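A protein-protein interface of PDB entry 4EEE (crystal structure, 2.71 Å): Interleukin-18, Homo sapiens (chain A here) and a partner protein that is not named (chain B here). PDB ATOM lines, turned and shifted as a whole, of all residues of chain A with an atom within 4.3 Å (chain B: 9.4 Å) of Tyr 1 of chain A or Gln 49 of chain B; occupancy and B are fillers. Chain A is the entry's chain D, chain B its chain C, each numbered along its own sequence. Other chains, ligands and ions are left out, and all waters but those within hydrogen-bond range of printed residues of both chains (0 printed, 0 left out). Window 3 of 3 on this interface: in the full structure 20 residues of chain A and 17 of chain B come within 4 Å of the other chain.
The side-chain hydroxyl (OH) of Tyr 38 of chain B lies within hydrogen-bond range of the backbone carbonyl oxygen (O) of Asp 54 of chain A (2.7 Å).
OD2 of Asp 48 of chain B lies within salt-bridge range of NZ of Lys 53 of chain A.
The side-chain amino group (NZ) of Lys 53 of chain A is in salt-bridge range of the side-chain carboxylate (OE1) of Glu 58 of chain B, at 2.7 Å.
The backbone NH (N) of Trp 39 of chain B is in hydrogen-bond range of the side-chain carboxylate (OE2) of Glu 58 of chain B (2.7 Å).
The side-chain amide oxygen of Gln 49 of chain B is in hydrogen-bond range of the side-chain hydroxyl of Thr 46 of chain B, 2.6 Å away.
The backbone NH of Tyr 1 of chain A lies within hydrogen-bond range of the side-chain hydroxyl of Ser 55 of chain A (2.9 Å).
The backbone NH of Tyr 1 of chain A sits at hydrogen-bond distance from the backbone carbonyl oxygen of Asp 94 of chain A, 3.0 Å away.
The backbone NH (N) of Lys 53 of chain A is in hydrogen-bond range of the backbone carbonyl oxygen (O) of Gly 3 of chain A.
Tyr 1 of chain A touches just these residues of chain B: Thr 46, Asp 48 and Gln 49.
Of chain A, only Tyr 1 and Ser 55 come within 4 Å of Gln 49 of chain B.
Asp 54 of chain A touches just these residues of chain B: Tyr 38 (2.7 Å) and Ile 40 (3.7 Å).
Of the printed residues of chain B, Lys 53 of chain A touches Tyr 38 (3.7 Å), Thr 46 (3.98 Å), Asp 48 (3.6 Å) and Glu 58 (2.7 Å).
Of the printed residues of chain B, Ser 55 of chain A touches Asn 44 and Gln 49.
Of the printed residues of chain A, Asp 48 of chain B touches Tyr 1 and Lys 53.
Val 47 of chain B touches none of the printed residues of chain A.
Gly 3 of chain A touches none of the printed residues of chain B.
The nearest printed residue of chain A that does not touch Gln 49 of chain B is Asp 54 of chain A (5.8 Å).
The nearest printed residue of chain A that does not touch Thr 46 of chain B is Ser 55 of chain A (4.1 Å).
Of the 9 printed residues of chain A, 4 touch a printed residue of chain B.
Of the 17 printed residues of chain B, 7 touch a printed residue of chain A.
Hydrophobic or aromatic side chains of chain B within 4 Å of the printed part of chain A: Tyr 38 and Ile 40.
Among the printed residues, 11 pairs touch across the chains.
Among the printed residues, pairs that only touch across the chains: Tyr 1 of chain A with Thr 46 of chain B, Tyr 1 of chain A with Asp 48 of chain B, Tyr 1 of chain A with Gln 49 of chain B, Lys 53 of chain A with Tyr 38 of chain B, Lys 53 of chain A with Thr 46 of chain B, Asp 54 of chain A with Ile 40 of chain B, Ser 55 of chain A with Asn 44 of chain B and Ser 55 of chain A with Gln 49 of chain B.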
ATOM      1  N   TYR A   1      13.848   9.886  -5.034  1.00  0.00           N
ATOM      2  CA  TYR A   1      15.066  10.210  -4.294  1.00  0.00           C
ATOM      3  C   TYR A   1      16.105  10.930  -5.149  1.00  0.00           C
ATOM      4  O   TYR A   1      16.353  10.550  -6.297  1.00  0.00           O
ATOM      5  CB  TYR A   1      15.684   8.941  -3.688  1.00  0.00           C
ATOM      6  CG  TYR A   1      16.905   9.227  -2.844  1.00  0.00           C
ATOM      7  CD1 TYR A   1      16.786   9.520  -1.492  1.00  0.00           C
ATOM      8  CD2 TYR A   1      18.175   9.218  -3.400  1.00  0.00           C
ATOM      9  CE1 TYR A   1      17.903   9.789  -0.714  1.00  0.00           C
ATOM     10  CE2 TYR A   1      19.296   9.484  -2.632  1.00  0.00           C
ATOM     11  CZ  TYR A   1      19.157   9.770  -1.289  1.00  0.00           C
ATOM     12  OH  TYR A   1      20.272  10.036  -0.522  1.00  0.00           O
ATOM     13  N   PHE A   2      16.705  11.968  -4.576  1.00  0.00           N
ATOM     14  CA  PHE A   2      17.754  12.717  -5.252  1.00  0.00           C
ATOM     15  C   PHE A   2      19.028  12.687  -4.417  1.00  0.00           C
ATOM     16  O   PHE A   2      19.022  13.048  -3.238  1.00  0.00           O
ATOM     17  CB  PHE A   2      17.322  14.165  -5.506  1.00  0.00           C
ATOM     18  CG  PHE A   2      16.238  14.309  -6.550  1.00  0.00           C
ATOM     19  CD1 PHE A   2      16.547  14.245  -7.902  1.00  0.00           C
ATOM     20  CD2 PHE A   2      14.916  14.514  -6.182  1.00  0.00           C
ATOM     21  CE1 PHE A   2      15.556  14.378  -8.867  1.00  0.00           C
ATOM     22  CE2 PHE A   2      13.924  14.653  -7.143  1.00  0.00           C
ATOM     23  CZ  PHE A   2      14.247  14.581  -8.488  1.00  0.00           C
ATOM     24  N   GLY A   3      20.119  12.256  -5.041  1.00  0.00           N
ATOM     25  CA  GLY A   3      21.389  12.144  -4.359  1.00  0.00           C
ATOM     26  C   GLY A   3      22.332  13.134  -5.004  1.00  0.00           C
ATOM     27  O   GLY A   3      22.516  13.141  -6.228  1.00  0.00           O
ATOM     28  N   LYS A  53      21.902  12.225  -8.522  1.00  0.00           N
ATOM     29  CA  LYS A  53      21.417  10.939  -9.004  1.00  0.00           C
ATOM     30  C   LYS A  53      19.946  10.745  -8.636  1.00  0.00           C
ATOM     31  O   LYS A  53      19.456  11.331  -7.667  1.00  0.00           O
ATOM     32  CB  LYS A  53      22.244   9.804  -8.426  1.00  0.00           C
ATOM     33  CG  LYS A  53      22.170   9.622  -6.932  1.00  0.00           C
ATOM     34  CD  LYS A  53      23.421   8.933  -6.408  1.00  0.00           C
ATOM     35  CE  LYS A  53      23.128   7.564  -5.835  1.00  0.00           C
ATOM     36  NZ  LYS A  53      24.373   6.951  -5.300  1.00  0.00           N
ATOM     37  N   ASP A  54      19.241   9.942  -9.427  1.00  0.00           N
ATOM     38  CA  ASP A  54      17.791   9.863  -9.337  1.00  0.00           C
ATOM     39  C   ASP A  54      17.294   8.423  -9.253  1.00  0.00           C
ATOM     40  O   ASP A  54      17.717   7.559 -10.025  1.00  0.00           O
ATOM     41  CB  ASP A  54      17.211  10.564 -10.573  1.00  0.00           C
ATOM     42  CG  ASP A  54      15.756  10.939 -10.407  1.00  0.00           C
ATOM     43  OD1 ASP A  54      15.134  10.539  -9.396  1.00  0.00           O
ATOM     44  OD2 ASP A  54      15.227  11.622 -11.306  1.00  0.00           O
ATOM     45  N   SER A  55      16.407   8.163  -8.296  1.00  0.00           N
ATOM     46  CA  SER A  55      15.783   6.849  -8.177  1.00  0.00           C
ATOM     47  C   SER A  55      14.884   6.583  -9.387  1.00  0.00           C
ATOM     48  O   SER A  55      14.708   5.440  -9.811  1.00  0.00           O
ATOM     49  CB  SER A  55      14.991   6.746  -6.877  1.00  0.00           C
ATOM     50  OG  SER A  55      13.916   7.662  -6.870  1.00  0.00           O
ATOM     51  N   ASN A  91      20.951  15.250   0.135  1.00  0.00           N
ATOM     52  CA  ASN A  91      19.929  14.368  -0.404  1.00  0.00           C
ATOM     53  C   ASN A  91      18.537  14.981  -0.294  1.00  0.00           C
ATOM     54  O   ASN A  91      18.236  15.704   0.657  1.00  0.00           O
ATOM     55  CB  ASN A  91      19.969  12.990   0.282  1.00  0.00           C
ATOM     56  CG  ASN A  91      19.465  13.027   1.710  1.00  0.00           C
ATOM     57  OD1 ASN A  91      18.253  13.020   1.955  1.00  0.00           O
ATOM     58  ND2 ASN A  91      20.390  13.049   2.663  1.00  0.00           N
ATOM     59  N   ILE A  92      17.688  14.656  -1.264  1.00  0.00           N
ATOM     60  CA  ILE A  92      16.288  15.053  -1.250  1.00  0.00           C
ATOM     61  C   ILE A  92      15.416  13.804  -1.338  1.00  0.00           C
ATOM     62  O   ILE A  92      15.486  13.059  -2.311  1.00  0.00           O
ATOM     63  CB  ILE A  92      15.952  15.981  -2.429  1.00  0.00           C
ATOM     64  CG1 ILE A  92      16.591  17.355  -2.228  1.00  0.00           C
ATOM     65  CG2 ILE A  92      14.447  16.111  -2.593  1.00  0.00           C
ATOM     66  CD1 ILE A  92      16.728  18.156  -3.503  1.00  0.00           C
ATOM     67  N   ASP A  94      12.414  12.855  -2.204  1.00  0.00           N
ATOM     68  CA  ASP A  94      11.178  13.064  -2.950  1.00  0.00           C
ATOM     69  C   ASP A  94      11.399  12.792  -4.431  1.00  0.00           C
ATOM     70  O   ASP A  94      12.532  12.613  -4.871  1.00  0.00           O
ATOM     71  CB  ASP A  94      10.672  14.492  -2.750  1.00  0.00           C
ATOM     72  CG  ASP A  94       9.164  14.591  -2.824  1.00  0.00           C
ATOM     73  OD1 ASP A  94       8.548  13.785  -3.551  1.00  0.00           O
ATOM     74  OD2 ASP A  94       8.592  15.476  -2.155  1.00  0.00           O
ATOM     75  N   TYR B  38      25.680   5.539 -12.143  1.00  0.00           N
ATOM     76  CA  TYR B  38      25.345   5.027 -10.825  1.00  0.00           C
ATOM     77  C   TYR B  38      24.381   3.854 -10.957  1.00  0.00           C
ATOM     78  O   TYR B  38      23.845   3.595 -12.032  1.00  0.00           O
ATOM     79  CB  TYR B  38      24.757   6.126  -9.937  1.00  0.00           C
ATOM     80  CG  TYR B  38      23.428   6.672 -10.405  1.00  0.00           C
ATOM     81  CD1 TYR B  38      23.359   7.597 -11.437  1.00  0.00           C
ATOM     82  CD2 TYR B  38      22.243   6.269  -9.808  1.00  0.00           C
ATOM     83  CE1 TYR B  38      22.147   8.101 -11.865  1.00  0.00           C
ATOM     84  CE2 TYR B  38      21.026   6.767 -10.230  1.00  0.00           C
ATOM     85  CZ  TYR B  38      20.984   7.683 -11.258  1.00  0.00           C
ATOM     86  OH  TYR B  38      19.775   8.182 -11.681  1.00  0.00           O
ATOM     87  N   TRP B  39      24.176   3.143  -9.856  1.00  0.00           N
ATOM     88  CA  TRP B  39      23.364   1.935  -9.846  1.00  0.00           C
ATOM     89  C   TRP B  39      21.959   2.108  -9.260  1.00  0.00           C
ATOM     90  O   TRP B  39      21.761   2.793  -8.250  1.00  0.00           O
ATOM     91  CB  TRP B  39      24.100   0.847  -9.060  1.00  0.00           C
ATOM     92  CG  TRP B  39      25.279   0.317  -9.791  1.00  0.00           C
ATOM     93  CD1 TRP B  39      26.565   0.779  -9.732  1.00  0.00           C
ATOM     94  CD2 TRP B  39      25.290  -0.783 -10.701  1.00  0.00           C
ATOM     95  NE1 TRP B  39      27.374   0.027 -10.551  1.00  0.00           N
ATOM     96  CE2 TRP B  39      26.614  -0.938 -11.160  1.00  0.00           C
ATOM     97  CE3 TRP B  39      24.308  -1.654 -11.174  1.00  0.00           C
ATOM     98  CZ2 TRP B  39      26.981  -1.935 -12.066  1.00  0.00           C
ATOM     99  CZ3 TRP B  39      24.670  -2.639 -12.075  1.00  0.00           C
ATOM    100  CH2 TRP B  39      25.994  -2.775 -12.511  1.00  0.00           C
ATOM    101  N   ILE B  40      20.990   1.459  -9.896  1.00  0.00           N
ATOM    102  CA  ILE B  40      19.671   1.278  -9.299  1.00  0.00           C
ATOM    103  C   ILE B  40      19.397  -0.203  -9.040  1.00  0.00           C
ATOM    104  O   ILE B  40      19.508  -1.035  -9.946  1.00  0.00           O
ATOM    105  CB  ILE B  40      18.558   1.865 -10.176  1.00  0.00           C
ATOM    106  CG1 ILE B  40      18.571   3.394 -10.071  1.00  0.00           C
ATOM    107  CG2 ILE B  40      17.203   1.305  -9.743  1.00  0.00           C
ATOM    108  CD1 ILE B  40      18.273   4.115 -11.375  1.00  0.00           C
ATOM    109  N   ILE B  41      19.042  -0.519  -7.797  1.00  0.00           N
ATOM    110  CA  ILE B  41      18.737  -1.890  -7.393  1.00  0.00           C
ATOM    111  C   ILE B  41      17.247  -2.167  -7.579  1.00  0.00           C
ATOM    112  O   ILE B  41      16.400  -1.388  -7.139  1.00  0.00           O
ATOM    113  CB  ILE B  41      19.143  -2.149  -5.921  1.00  0.00           C
ATOM    114  CG1 ILE B  41      20.526  -1.558  -5.658  1.00  0.00           C
ATOM    115  CG2 ILE B  41      19.108  -3.644  -5.594  1.00  0.00           C
ATOM    116  CD1 ILE B  41      21.594  -2.065  -6.621  1.00  0.00           C
ATOM    117  N   LYS B  43      13.812  -1.897  -8.935  1.00  0.00           N
ATOM    118  CA  LYS B  43      12.968  -0.998  -9.727  1.00  0.00           C
ATOM    119  C   LYS B  43      13.285   0.494  -9.614  1.00  0.00           C
ATOM    120  O   LYS B  43      13.289   1.203 -10.609  1.00  0.00           O
ATOM    121  CB  LYS B  43      11.490  -1.236  -9.360  1.00  0.00           C
ATOM    122  CG  LYS B  43      10.488  -0.568 -10.291  1.00  0.00           C
ATOM    123  N   ASN B  44      13.545   0.970  -8.403  1.00  0.00           N
ATOM    124  CA  ASN B  44      13.615   2.411  -8.161  1.00  0.00           C
ATOM    125  C   ASN B  44      14.490   2.804  -6.978  1.00  0.00           C
ATOM    126  O   ASN B  44      14.343   3.904  -6.433  1.00  0.00           O
ATOM    127  CB  ASN B  44      12.197   2.920  -7.935  1.00  0.00           C
ATOM    128  CG  ASN B  44      11.539   2.271  -6.735  1.00  0.00           C
ATOM    129  OD1 ASN B  44      11.751   1.095  -6.441  1.00  0.00           O
ATOM    130  ND2 ASN B  44      10.744   3.045  -6.028  1.00  0.00           N
ATOM    131  N   LYS B  45      15.391   1.913  -6.578  1.00  0.00           N
ATOM    132  CA  LYS B  45      16.175   2.124  -5.363  1.00  0.00           C
ATOM    133  C   LYS B  45      17.665   2.325  -5.606  1.00  0.00           C
ATOM    134  O   LYS B  45      18.377   1.394  -6.002  1.00  0.00           O
ATOM    135  CB  LYS B  45      15.986   0.901  -4.453  1.00  0.00           C
ATOM    136  N   THR B  46      18.143   3.539  -5.363  1.00  0.00           N
ATOM    137  CA  THR B  46      19.584   3.765  -5.332  1.00  0.00           C
ATOM    138  C   THR B  46      20.142   3.017  -4.137  1.00  0.00           C
ATOM    139  O   THR B  46      19.406   2.682  -3.208  1.00  0.00           O
ATOM    140  CB  THR B  46      19.942   5.254  -5.230  1.00  0.00           C
ATOM    141  OG1 THR B  46      19.352   5.810  -4.048  1.00  0.00           O
ATOM    142  CG2 THR B  46      19.464   6.021  -6.472  1.00  0.00           C
ATOM    143  N   VAL B  47      21.441   2.754  -4.153  1.00  0.00           N
ATOM    144  CA  VAL B  47      22.051   2.008  -3.064  1.00  0.00           C
ATOM    145  C   VAL B  47      21.886   2.754  -1.744  1.00  0.00           C
ATOM    146  O   VAL B  47      21.694   2.138  -0.691  1.00  0.00           O
ATOM    147  CB  VAL B  47      23.523   1.698  -3.349  1.00  0.00           C
ATOM    148  CG1 VAL B  47      24.151   0.982  -2.163  1.00  0.00           C
ATOM    149  CG2 VAL B  47      23.633   0.849  -4.613  1.00  0.00           C
ATOM    150  N   ASP B  48      21.930   4.081  -1.811  1.00  0.00           N
ATOM    151  CA  ASP B  48      21.723   4.915  -0.638  1.00  0.00           C
ATOM    152  C   ASP B  48      20.399   4.554   0.024  1.00  0.00           C
ATOM    153  O   ASP B  48      20.257   4.632   1.245  1.00  0.00           O
ATOM    154  CB  ASP B  48      21.713   6.400  -1.029  1.00  0.00           C
ATOM    155  CG  ASP B  48      23.089   6.912  -1.426  1.00  0.00           C
ATOM    156  OD1 ASP B  48      24.087   6.220  -1.132  1.00  0.00           O
ATOM    157  OD2 ASP B  48      23.176   8.000  -2.038  1.00  0.00           O
ATOM    158  N   GLN B  49      19.430   4.151  -0.791  1.00  0.00           N
ATOM    159  CA  GLN B  49      18.057   3.954  -0.321  1.00  0.00           C
ATOM    160  C   GLN B  49      17.854   2.619   0.382  1.00  0.00           C
ATOM    161  O   GLN B  49      16.763   2.323   0.872  1.00  0.00           O
ATOM    162  CB  GLN B  49      17.071   4.059  -1.494  1.00  0.00           C
ATOM    163  CG  GLN B  49      16.634   5.485  -1.827  1.00  0.00           C
ATOM    164  CD  GLN B  49      16.023   5.574  -3.216  1.00  0.00           C
ATOM    165  OE1 GLN B  49      16.742   5.592  -4.217  1.00  0.00           O
ATOM    166  NE2 GLN B  49      14.692   5.630  -3.283  1.00  0.00           N
ATOM    167  N   LEU B  50      18.904   1.811   0.433  1.00  0.00           N
ATOM    168  CA  LEU B  50      18.773   0.445   0.929  1.00  0.00           C
ATOM    169  C   LEU B  50      18.907   0.307   2.447  1.00  0.00           C
ATOM    170  O   LEU B  50      19.571   1.120   3.101  1.00  0.00           O
ATOM    171  CB  LEU B  50      19.798  -0.449   0.224  1.00  0.00           C
ATOM    172  CG  LEU B  50      19.594  -0.594  -1.283  1.00  0.00           C
ATOM    173  CD1 LEU B  50      20.774  -1.291  -1.932  1.00  0.00           C
ATOM    174  CD2 LEU B  50      18.293  -1.337  -1.585  1.00  0.00           C
ATOM    175  N   PRO B  51      18.273  -0.735   3.006  1.00  0.00           N
ATOM    176  CA  PRO B  51      18.475  -1.099   4.411  1.00  0.00           C
ATOM    177  C   PRO B  51      19.964  -1.309   4.643  1.00  0.00           C
ATOM    178  O   PRO B  51      20.632  -1.879   3.778  1.00  0.00           O
ATOM    179  CB  PRO B  51      17.728  -2.434   4.569  1.00  0.00           C
ATOM    180  CG  PRO B  51      17.054  -2.710   3.282  1.00  0.00           C
ATOM    181  CD  PRO B  51      17.291  -1.591   2.321  1.00  0.00           C
ATOM    182  N   PRO B  52      20.489  -0.840   5.792  1.00  0.00           N
ATOM    183  CA  PRO B  52      21.931  -0.930   6.079  1.00  0.00           C
ATOM    184  C   PRO B  52      22.374  -2.383   6.241  1.00  0.00           C
ATOM    185  O   PRO B  52      21.614  -3.199   6.766  1.00  0.00           O
ATOM    186  CB  PRO B  52      22.072  -0.177   7.407  1.00  0.00           C
ATOM    187  CG  PRO B  52      20.730  -0.310   8.057  1.00  0.00           C
ATOM    188  CD  PRO B  52      19.736  -0.271   6.927  1.00  0.00           C
ATOM    189  N   SER B  54      22.859  -4.574   3.673  1.00  0.00           N
ATOM    190  CA  SER B  54      22.011  -5.347   2.774  1.00  0.00           C
ATOM    191  C   SER B  54      22.816  -6.164   1.776  1.00  0.00           C
ATOM    192  O   SER B  54      22.264  -6.976   1.031  1.00  0.00           O
ATOM    193  CB  SER B  54      21.108  -4.391   2.010  1.00  0.00           C
ATOM    194  OG  SER B  54      21.861  -3.615   1.080  1.00  0.00           O
ATOM    195  N   TYR B  56      24.805  -4.803  -0.616  1.00  0.00           N
ATOM    196  CA  TYR B  56      25.172  -3.940  -1.736  1.00  0.00           C
ATOM    197  C   TYR B  56      26.066  -2.803  -1.267  1.00  0.00           C
ATOM    198  O   TYR B  56      25.835  -2.216  -0.210  1.00  0.00           O
ATOM    199  CB  TYR B  56      23.922  -3.360  -2.417  1.00  0.00           C
ATOM    200  CG  TYR B  56      23.027  -4.391  -3.069  1.00  0.00           C
ATOM    201  CD1 TYR B  56      23.242  -4.802  -4.377  1.00  0.00           C
ATOM    202  CD2 TYR B  56      21.968  -4.955  -2.375  1.00  0.00           C
ATOM    203  CE1 TYR B  56      22.424  -5.755  -4.975  1.00  0.00           C
ATOM    204  CE2 TYR B  56      21.148  -5.908  -2.962  1.00  0.00           C
ATOM    205  CZ  TYR B  56      21.380  -6.304  -4.260  1.00  0.00           C
ATOM    206  OH  TYR B  56      20.562  -7.250  -4.835  1.00  0.00           O
ATOM    207  N   GLU B  58      28.137   0.666  -3.153  1.00  0.00           N
ATOM    208  CA  GLU B  58      28.443   1.416  -4.364  1.00  0.00           C
ATOM    209  C   GLU B  58      29.714   2.236  -4.183  1.00  0.00           C
ATOM    210  O   GLU B  58      29.890   2.923  -3.174  1.00  0.00           O
ATOM    211  CB  GLU B  58      27.267   2.325  -4.761  1.00  0.00           C
ATOM    212  CG  GLU B  58      27.400   2.971  -6.146  1.00  0.00           C
ATOM    213  CD  GLU B  58      26.167   3.774  -6.554  1.00  0.00           C
ATOM    214  OE1 GLU B  58      25.772   4.696  -5.803  1.00  0.00           O
ATOM    215  OE2 GLU B  58      25.598   3.491  -7.633  1.00  0.00           O
